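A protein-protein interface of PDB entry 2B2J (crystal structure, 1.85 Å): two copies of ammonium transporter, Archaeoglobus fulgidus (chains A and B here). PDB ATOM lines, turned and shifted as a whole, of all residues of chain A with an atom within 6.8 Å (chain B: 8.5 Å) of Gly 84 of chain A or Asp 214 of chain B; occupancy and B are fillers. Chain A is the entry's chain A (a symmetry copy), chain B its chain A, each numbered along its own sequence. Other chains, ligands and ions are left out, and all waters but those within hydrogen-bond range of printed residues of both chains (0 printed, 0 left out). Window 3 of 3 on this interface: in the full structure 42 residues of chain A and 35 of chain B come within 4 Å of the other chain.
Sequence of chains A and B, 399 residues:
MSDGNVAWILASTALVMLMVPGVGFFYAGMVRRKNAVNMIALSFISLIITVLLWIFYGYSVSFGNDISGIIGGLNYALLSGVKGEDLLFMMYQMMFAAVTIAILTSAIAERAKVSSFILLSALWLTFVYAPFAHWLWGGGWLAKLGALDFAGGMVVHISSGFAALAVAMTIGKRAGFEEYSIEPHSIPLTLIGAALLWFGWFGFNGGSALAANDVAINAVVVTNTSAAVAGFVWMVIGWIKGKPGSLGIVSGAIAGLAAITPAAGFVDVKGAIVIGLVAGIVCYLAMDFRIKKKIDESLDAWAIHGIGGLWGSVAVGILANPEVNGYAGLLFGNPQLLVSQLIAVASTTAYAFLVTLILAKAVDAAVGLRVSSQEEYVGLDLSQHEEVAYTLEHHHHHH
The side-chain amide oxygen (OD1) of Asn 5 of chain B lies within hydrogen-bond range of the backbone NH (N) of Ala 212 of chain B (3.0 Å).
Val 6 of chain A touches Ala 212 of chain B (CB to O, 3.7 Å). CG1 of Val 6 of chain A touches CD1 of Ile 217 of chain B, 3.9 Å away. Gly 84 of chain A touches Asp 214 of chain B. Ile 217 of chain B touches Leu 87 of chain A (CG2 to CB, 3.8 Å). CG2 of Ile 217 of chain B touches N of Leu 88 of chain A, at 3.7 Å.
Of the printed residues of chain B, Leu 87 of chain A touches Ile 217 (3.8 Å). Ala 209 of chain B touches none of the printed residues of chain A. Of the printed residues of chain A, Ala 212 of chain B touches Val 6 (3.7 Å). Of the printed residues of chain A, Asp 214 of chain B touches Gly 84 (3.95 Å). Of the printed residues of chain A, Ile 217 of chain B touches Val 6 (3.9 Å), Leu 87 (3.8 Å) and Leu 88 (3.7 Å). The nearest printed residue of chain B that does not touch Val 6 of chain A is Asn 213 of chain B (4.4 Å).
Printed residues of chain B that touch a printed residue of chain A: Ala 212, Asp 214 and Ile 217. Of the 9 printed residues of chain A, 4 touch a printed residue of chain B. Among the printed residues, no Asp or Glu carboxylate lies within 4 Å of a Lys or Arg side-chain nitrogen of the other chain.
No position is printed for both chains. Of the 5 pairs that touch across the chains among the printed residues, none has its exchanged pair printed and touching as well.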
ATOM      1  N   VAL A   6     -33.023  -5.487  21.260  1.00  0.00           N
ATOM      2  CA  VAL A   6     -32.203  -6.684  21.183  1.00  0.00           C
ATOM      3  C   VAL A   6     -31.025  -6.523  22.148  1.00  0.00           C
ATOM      4  O   VAL A   6     -30.607  -7.478  22.807  1.00  0.00           O
ATOM      5  CB  VAL A   6     -31.675  -6.911  19.750  1.00  0.00           C
ATOM      6  CG1 VAL A   6     -30.792  -8.149  19.707  1.00  0.00           C
ATOM      7  CG2 VAL A   6     -32.846  -7.056  18.796  1.00  0.00           C
ATOM      8  N   VAL A  82     -36.591 -22.212  14.037  1.00  0.00           N
ATOM      9  CA  VAL A  82     -36.526 -21.098  14.987  1.00  0.00           C
ATOM     10  C   VAL A  82     -35.484 -20.102  14.480  1.00  0.00           C
ATOM     11  O   VAL A  82     -34.311 -20.445  14.352  1.00  0.00           O
ATOM     12  CB  VAL A  82     -36.115 -21.579  16.398  1.00  0.00           C
ATOM     13  CG1 VAL A  82     -36.233 -20.431  17.393  1.00  0.00           C
ATOM     14  CG2 VAL A  82     -36.979 -22.754  16.820  1.00  0.00           C
ATOM     15  N   LYS A  83     -35.901 -18.874  14.187  1.00  0.00           N
ATOM     16  CA  LYS A  83     -34.953 -17.884  13.682  1.00  0.00           C
ATOM     17  C   LYS A  83     -35.172 -16.452  14.149  1.00  0.00           C
ATOM     18  O   LYS A  83     -36.220 -16.109  14.697  1.00  0.00           O
ATOM     19  CB  LYS A  83     -34.946 -17.897  12.156  1.00  0.00           C
ATOM     20  CG  LYS A  83     -34.476 -19.199  11.544  1.00  0.00           C
ATOM     21  CD  LYS A  83     -34.382 -19.073  10.033  1.00  0.00           C
ATOM     22  CE  LYS A  83     -33.792 -20.327   9.406  1.00  0.00           C
ATOM     23  NZ  LYS A  83     -33.554 -20.159   7.939  1.00  0.00           N
ATOM     24  N   GLY A  84     -34.162 -15.620  13.910  1.00  0.00           N
ATOM     25  CA  GLY A  84     -34.231 -14.220  14.287  1.00  0.00           C
ATOM     26  C   GLY A  84     -34.685 -14.006  15.716  1.00  0.00           C
ATOM     27  O   GLY A  84     -34.070 -14.512  16.654  1.00  0.00           O
ATOM     28  N   GLU A  85     -35.763 -13.247  15.877  1.00  0.00           N
ATOM     29  CA  GLU A  85     -36.304 -12.960  17.195  1.00  0.00           C
ATOM     30  C   GLU A  85     -36.531 -14.208  18.024  1.00  0.00           C
ATOM     31  O   GLU A  85     -36.199 -14.246  19.204  1.00  0.00           O
ATOM     32  CB  GLU A  85     -37.628 -12.221  17.079  1.00  0.00           C
ATOM     33  CG  GLU A  85     -37.501 -10.734  16.874  1.00  0.00           C
ATOM     34  CD  GLU A  85     -38.764 -10.002  17.296  1.00  0.00           C
ATOM     35  OE1 GLU A  85     -39.841 -10.287  16.714  1.00  0.00           O
ATOM     36  OE2 GLU A  85     -38.675  -9.152  18.214  1.00  0.00           O
ATOM     37  N   ASP A  86     -37.123 -15.220  17.400  1.00  0.00           N
ATOM     38  CA  ASP A  86     -37.412 -16.473  18.081  1.00  0.00           C
ATOM     39  C   ASP A  86     -36.183 -17.056  18.750  1.00  0.00           C
ATOM     40  O   ASP A  86     -36.263 -17.569  19.865  1.00  0.00           O
ATOM     41  CB  ASP A  86     -37.978 -17.486  17.094  1.00  0.00           C
ATOM     42  CG  ASP A  86     -39.320 -17.066  16.544  1.00  0.00           C
ATOM     43  OD1 ASP A  86     -39.876 -17.826  15.725  1.00  0.00           O
ATOM     44  OD2 ASP A  86     -39.817 -15.982  16.930  1.00  0.00           O
ATOM     45  N   LEU A  87     -35.048 -16.989  18.061  1.00  0.00           N
ATOM     46  CA  LEU A  87     -33.801 -17.505  18.610  1.00  0.00           C
ATOM     47  C   LEU A  87     -33.455 -16.799  19.912  1.00  0.00           C
ATOM     48  O   LEU A  87     -33.107 -17.442  20.902  1.00  0.00           O
ATOM     49  CB  LEU A  87     -32.666 -17.318  17.612  1.00  0.00           C
ATOM     50  CG  LEU A  87     -32.604 -18.384  16.531  1.00  0.00           C
ATOM     51  CD1 LEU A  87     -31.518 -18.029  15.539  1.00  0.00           C
ATOM     52  CD2 LEU A  87     -32.328 -19.733  17.174  1.00  0.00           C
ATOM     53  N   LEU A  88     -33.551 -15.475  19.911  1.00  0.00           N
ATOM     54  CA  LEU A  88     -33.239 -14.714  21.106  1.00  0.00           C
ATOM     55  C   LEU A  88     -34.214 -15.114  22.204  1.00  0.00           C
ATOM     56  O   LEU A  88     -33.816 -15.353  23.347  1.00  0.00           O
ATOM     57  CB  LEU A  88     -33.326 -13.204  20.831  1.00  0.00           C
ATOM     58  CG  LEU A  88     -32.982 -12.264  22.000  1.00  0.00           C
ATOM     59  CD1 LEU A  88     -31.678 -12.676  22.639  1.00  0.00           C
ATOM     60  CD2 LEU A  88     -32.892 -10.834  21.501  1.00  0.00           C
ATOM     61  N   PHE A  89     -35.490 -15.207  21.846  1.00  0.00           N
ATOM     62  CA  PHE A  89     -36.514 -15.582  22.803  1.00  0.00           C
ATOM     63  C   PHE A  89     -36.219 -16.966  23.356  1.00  0.00           C
ATOM     64  O   PHE A  89     -36.255 -17.192  24.563  1.00  0.00           O
ATOM     65  CB  PHE A  89     -37.879 -15.582  22.126  1.00  0.00           C
ATOM     66  CG  PHE A  89     -39.004 -15.990  23.033  1.00  0.00           C
ATOM     67  CD1 PHE A  89     -39.436 -15.147  24.051  1.00  0.00           C
ATOM     68  CD2 PHE A  89     -39.629 -17.222  22.874  1.00  0.00           C
ATOM     69  CE1 PHE A  89     -40.472 -15.526  24.895  1.00  0.00           C
ATOM     70  CE2 PHE A  89     -40.666 -17.608  23.712  1.00  0.00           C
ATOM     71  CZ  PHE A  89     -41.088 -16.756  24.725  1.00  0.00           C
ATOM     72  N   ASN B   5     -27.088  -0.475  19.210  1.00  0.00           N
ATOM     73  CA  ASN B   5     -25.799  -1.063  18.894  1.00  0.00           C
ATOM     74  C   ASN B   5     -24.703  -0.581  19.814  1.00  0.00           C
ATOM     75  O   ASN B   5     -23.812  -1.341  20.176  1.00  0.00           O
ATOM     76  CB  ASN B   5     -25.412  -0.785  17.447  1.00  0.00           C
ATOM     77  CG  ASN B   5     -26.285  -1.535  16.463  1.00  0.00           C
ATOM     78  OD1 ASN B   5     -26.924  -2.534  16.815  1.00  0.00           O
ATOM     79  ND2 ASN B   5     -26.308  -1.069  15.218  1.00  0.00           N
ATOM     80  N   PHE B 150     -14.285 -15.264  13.872  1.00  0.00           N
ATOM     81  CA  PHE B 150     -15.351 -14.460  14.430  1.00  0.00           C
ATOM     82  C   PHE B 150     -15.039 -13.757  15.746  1.00  0.00           C
ATOM     83  O   PHE B 150     -15.068 -12.527  15.809  1.00  0.00           O
ATOM     84  CB  PHE B 150     -16.622 -15.287  14.589  1.00  0.00           C
ATOM     85  CG  PHE B 150     -17.824 -14.463  14.949  1.00  0.00           C
ATOM     86  CD1 PHE B 150     -18.423 -13.642  14.004  1.00  0.00           C
ATOM     87  CD2 PHE B 150     -18.324 -14.465  16.252  1.00  0.00           C
ATOM     88  CE1 PHE B 150     -19.495 -12.829  14.342  1.00  0.00           C
ATOM     89  CE2 PHE B 150     -19.397 -13.656  16.603  1.00  0.00           C
ATOM     90  CZ  PHE B 150     -19.983 -12.835  15.642  1.00  0.00           C
ATOM     91  N   GLY B 206     -20.852 -12.764  21.482  1.00  0.00           N
ATOM     92  CA  GLY B 206     -22.025 -11.988  21.118  1.00  0.00           C
ATOM     93  C   GLY B 206     -21.751 -10.537  20.773  1.00  0.00           C
ATOM     94  O   GLY B 206     -22.507  -9.908  20.029  1.00  0.00           O
ATOM     95  N   ALA B 209     -20.243  -9.250  16.904  1.00  0.00           N
ATOM     96  CA  ALA B 209     -21.024  -8.917  15.713  1.00  0.00           C
ATOM     97  C   ALA B 209     -21.002  -7.405  15.552  1.00  0.00           C
ATOM     98  O   ALA B 209     -21.379  -6.864  14.512  1.00  0.00           O
ATOM     99  CB  ALA B 209     -22.465  -9.405  15.859  1.00  0.00           C
ATOM    100  N   ALA B 211     -22.875  -5.347  16.751  1.00  0.00           N
ATOM    101  CA  ALA B 211     -24.233  -4.822  16.670  1.00  0.00           C
ATOM    102  C   ALA B 211     -25.210  -5.780  17.336  1.00  0.00           C
ATOM    103  O   ALA B 211     -24.987  -6.992  17.355  1.00  0.00           O
ATOM    104  CB  ALA B 211     -24.630  -4.617  15.217  1.00  0.00           C
ATOM    105  N   ALA B 212     -26.287  -5.231  17.895  1.00  0.00           N
ATOM    106  CA  ALA B 212     -27.303  -6.056  18.538  1.00  0.00           C
ATOM    107  C   ALA B 212     -28.173  -6.503  17.371  1.00  0.00           C
ATOM    108  O   ALA B 212     -29.231  -5.935  17.117  1.00  0.00           O
ATOM    109  CB  ALA B 212     -28.108  -5.224  19.538  1.00  0.00           C
ATOM    110  N   ASN B 213     -27.699  -7.514  16.652  1.00  0.00           N
ATOM    111  CA  ASN B 213     -28.393  -8.021  15.480  1.00  0.00           C
ATOM    112  C   ASN B 213     -28.567  -9.530  15.512  1.00  0.00           C
ATOM    113  O   ASN B 213     -28.366 -10.178  16.544  1.00  0.00           O
ATOM    114  CB  ASN B 213     -27.607  -7.649  14.228  1.00  0.00           C
ATOM    115  CG  ASN B 213     -26.250  -8.343  14.160  1.00  0.00           C
ATOM    116  OD1 ASN B 213     -25.432  -8.041  13.293  1.00  0.00           O
ATOM    117  ND2 ASN B 213     -26.011  -9.280  15.071  1.00  0.00           N
ATOM    118  N   ASP B 214     -28.911 -10.091  14.357  1.00  0.00           N
ATOM    119  CA  ASP B 214     -29.115 -11.524  14.246  1.00  0.00           C
ATOM    120  C   ASP B 214     -27.819 -12.326  14.376  1.00  0.00           C
ATOM    121  O   ASP B 214     -27.824 -13.425  14.938  1.00  0.00           O
ATOM    122  CB  ASP B 214     -29.834 -11.847  12.930  1.00  0.00           C
ATOM    123  CG  ASP B 214     -31.333 -11.542  12.992  1.00  0.00           C
ATOM    124  OD1 ASP B 214     -32.038 -11.748  11.977  1.00  0.00           O
ATOM    125  OD2 ASP B 214     -31.813 -11.101  14.061  1.00  0.00           O
ATOM    126  N   VAL B 215     -26.711 -11.787  13.875  1.00  0.00           N
ATOM    127  CA  VAL B 215     -25.439 -12.497  13.983  1.00  0.00           C
ATOM    128  C   VAL B 215     -25.085 -12.667  15.456  1.00  0.00           C
ATOM    129  O   VAL B 215     -24.710 -13.753  15.896  1.00  0.00           O
ATOM    130  CB  VAL B 215     -24.300 -11.733  13.280  1.00  0.00           C
ATOM    131  CG1 VAL B 215     -22.966 -12.440  13.510  1.00  0.00           C
ATOM    132  CG2 VAL B 215     -24.594 -11.646  11.798  1.00  0.00           C
ATOM    133  N   ALA B 216     -25.214 -11.585  16.215  1.00  0.00           N
ATOM    134  CA  ALA B 216     -24.912 -11.616  17.639  1.00  0.00           C
ATOM    135  C   ALA B 216     -25.793 -12.668  18.301  1.00  0.00           C
ATOM    136  O   ALA B 216     -25.312 -13.518  19.058  1.00  0.00           O
ATOM    137  CB  ALA B 216     -25.164 -10.245  18.254  1.00  0.00           C
ATOM    138  N   ILE B 217     -27.088 -12.611  17.998  1.00  0.00           N
ATOM    139  CA  ILE B 217     -28.056 -13.559  18.537  1.00  0.00           C
ATOM    140  C   ILE B 217     -27.632 -14.996  18.229  1.00  0.00           C
ATOM    141  O   ILE B 217     -27.677 -15.869  19.096  1.00  0.00           O
ATOM    142  CB  ILE B 217     -29.449 -13.297  17.949  1.00  0.00           C
ATOM    143  CG1 ILE B 217     -29.974 -11.957  18.457  1.00  0.00           C
ATOM    144  CG2 ILE B 217     -30.398 -14.407  18.328  1.00  0.00           C
ATOM    145  CD1 ILE B 217     -31.343 -11.600  17.909  1.00  0.00           C
ATOM    146  N   ASN B 218     -27.211 -15.241  16.995  1.00  0.00           N
ATOM    147  CA  ASN B 218     -26.767 -16.568  16.620  1.00  0.00           C
ATOM    148  C   ASN B 218     -25.510 -16.899  17.409  1.00  0.00           C
ATOM    149  O   ASN B 218     -25.383 -17.987  17.964  1.00  0.00           O
ATOM    150  CB  ASN B 218     -26.479 -16.618  15.120  1.00  0.00           C
ATOM    151  CG  ASN B 218     -26.013 -17.985  14.659  1.00  0.00           C
ATOM    152  OD1 ASN B 218     -24.827 -18.321  14.757  1.00  0.00           O
ATOM    153  ND2 ASN B 218     -26.946 -18.789  14.161  1.00  0.00           N
ATOM    154  N   ALA B 219     -24.585 -15.950  17.479  1.00  0.00           N
ATOM    155  CA  ALA B 219     -23.340 -16.176  18.207  1.00  0.00           C
ATOM    156  C   ALA B 219     -23.653 -16.603  19.631  1.00  0.00           C
ATOM    157  O   ALA B 219     -23.066 -17.556  20.148  1.00  0.00           O
ATOM    158  CB  ALA B 219     -22.492 -14.910  18.211  1.00  0.00           C
ATOM    159  N   VAL B 220     -24.594 -15.909  20.263  1.00  0.00           N
ATOM    160  CA  VAL B 220     -24.955 -16.227  21.640  1.00  0.00           C
ATOM    161  C   VAL B 220     -25.545 -17.627  21.761  1.00  0.00           C
ATOM    162  O   VAL B 220     -25.245 -18.365  22.705  1.00  0.00           O
ATOM    163  CB  VAL B 220     -25.959 -15.195  22.210  1.00  0.00           C
ATOM    164  CG1 VAL B 220     -26.519 -15.683  23.535  1.00  0.00           C
ATOM    165  CG2 VAL B 220     -25.269 -13.848  22.397  1.00  0.00           C
ATOM    166  N   VAL B 221     -26.387 -17.998  20.807  1.00  0.00           N
ATOM    167  CA  VAL B 221     -27.001 -19.319  20.839  1.00  0.00           C
ATOM    168  C   VAL B 221     -25.945 -20.422  20.689  1.00  0.00           C
ATOM    169  O   VAL B 221     -25.831 -21.315  21.532  1.00  0.00           O
ATOM    170  CB  VAL B 221     -28.048 -19.473  19.707  1.00  0.00           C
ATOM    171  CG1 VAL B 221     -28.620 -20.872  19.719  1.00  0.00           C
ATOM    172  CG2 VAL B 221     -29.156 -18.454  19.876  1.00  0.00           C
ATOM    173  N   ALA B 264     -18.507 -18.611  16.201  1.00  0.00           N
ATOM    174  CA  ALA B 264     -19.765 -18.144  16.777  1.00  0.00           C
ATOM    175  C   ALA B 264     -20.733 -17.485  15.799  1.00  0.00           C
ATOM    176  O   ALA B 264     -21.926 -17.762  15.835  1.00  0.00           O
ATOM    177  CB  ALA B 264     -19.487 -17.204  17.935  1.00  0.00           C
ATOM    178  N   GLY B 265     -20.228 -16.627  14.919  1.00  0.00           N
ATOM    179  CA  GLY B 265     -21.113 -15.945  13.992  1.00  0.00           C
ATOM    180  C   GLY B 265     -21.307 -16.494  12.589  1.00  0.00           C
ATOM    181  O   GLY B 265     -21.949 -15.839  11.767  1.00  0.00           O
ATOM    182  N   VAL B 267     -21.664 -20.363  11.941  1.00  0.00           N
ATOM    183  CA  VAL B 267     -22.287 -21.686  11.934  1.00  0.00           C
ATOM    184  C   VAL B 267     -23.693 -21.754  12.533  1.00  0.00           C
ATOM    185  O   VAL B 267     -24.147 -20.824  13.206  1.00  0.00           O
ATOM    186  CB  VAL B 267     -21.385 -22.713  12.673  1.00  0.00           C
ATOM    187  CG1 VAL B 267     -19.993 -22.722  12.057  1.00  0.00           C
ATOM    188  CG2 VAL B 267     -21.299 -22.370  14.152  1.00  0.00           C
ATOM    189  N   GLU B 323     -26.306 -19.821   5.084  1.00  0.00           N
ATOM    190  CA  GLU B 323     -27.621 -19.545   5.611  1.00  0.00           C
ATOM    191  C   GLU B 323     -27.442 -18.644   6.823  1.00  0.00           C
ATOM    192  O   GLU B 323     -28.134 -17.639   6.981  1.00  0.00           O
ATOM    193  CB  GLU B 323     -28.280 -20.858   6.033  1.00  0.00           C
ATOM    194  CG  GLU B 323     -29.789 -20.893   5.915  1.00  0.00           C
ATOM    195  CD  GLU B 323     -30.249 -20.927   4.472  1.00  0.00           C
ATOM    196  OE1 GLU B 323     -29.875 -21.882   3.754  1.00  0.00           O
ATOM    197  OE2 GLU B 323     -30.981 -19.999   4.059  1.00  0.00           O
ATOM    198  N   VAL B 324     -26.494 -19.004   7.676  1.00  0.00           N
ATOM    199  CA  VAL B 324     -26.257 -18.236   8.879  1.00  0.00           C
ATOM    200  C   VAL B 324     -25.709 -16.843   8.633  1.00  0.00           C
ATOM    201  O   VAL B 324     -26.371 -15.854   8.938  1.00  0.00           O
ATOM    202  CB  VAL B 324     -25.300 -18.973   9.826  1.00  0.00           C
ATOM    203  CG1 VAL B 324     -24.967 -18.098  11.022  1.00  0.00           C
ATOM    204  CG2 VAL B 324     -25.939 -20.259  10.287  1.00  0.00           C
ATOM    205  N   ASN B 325     -24.510 -16.751   8.074  1.00  0.00           N
ATOM    206  CA  ASN B 325     -23.918 -15.441   7.873  1.00  0.00           C
ATOM    207  C   ASN B 325     -23.266 -15.242   6.509  1.00  0.00           C
ATOM    208  O   ASN B 325     -22.234 -14.579   6.395  1.00  0.00           O
ATOM    209  CB  ASN B 325     -22.906 -15.182   8.996  1.00  0.00           C
ATOM    210  CG  ASN B 325     -22.579 -13.715   9.164  1.00  0.00           C
ATOM    211  OD1 ASN B 325     -23.299 -12.852   8.675  1.00  0.00           O
ATOM    212  ND2 ASN B 325     -21.496 -13.424   9.874  1.00  0.00           N
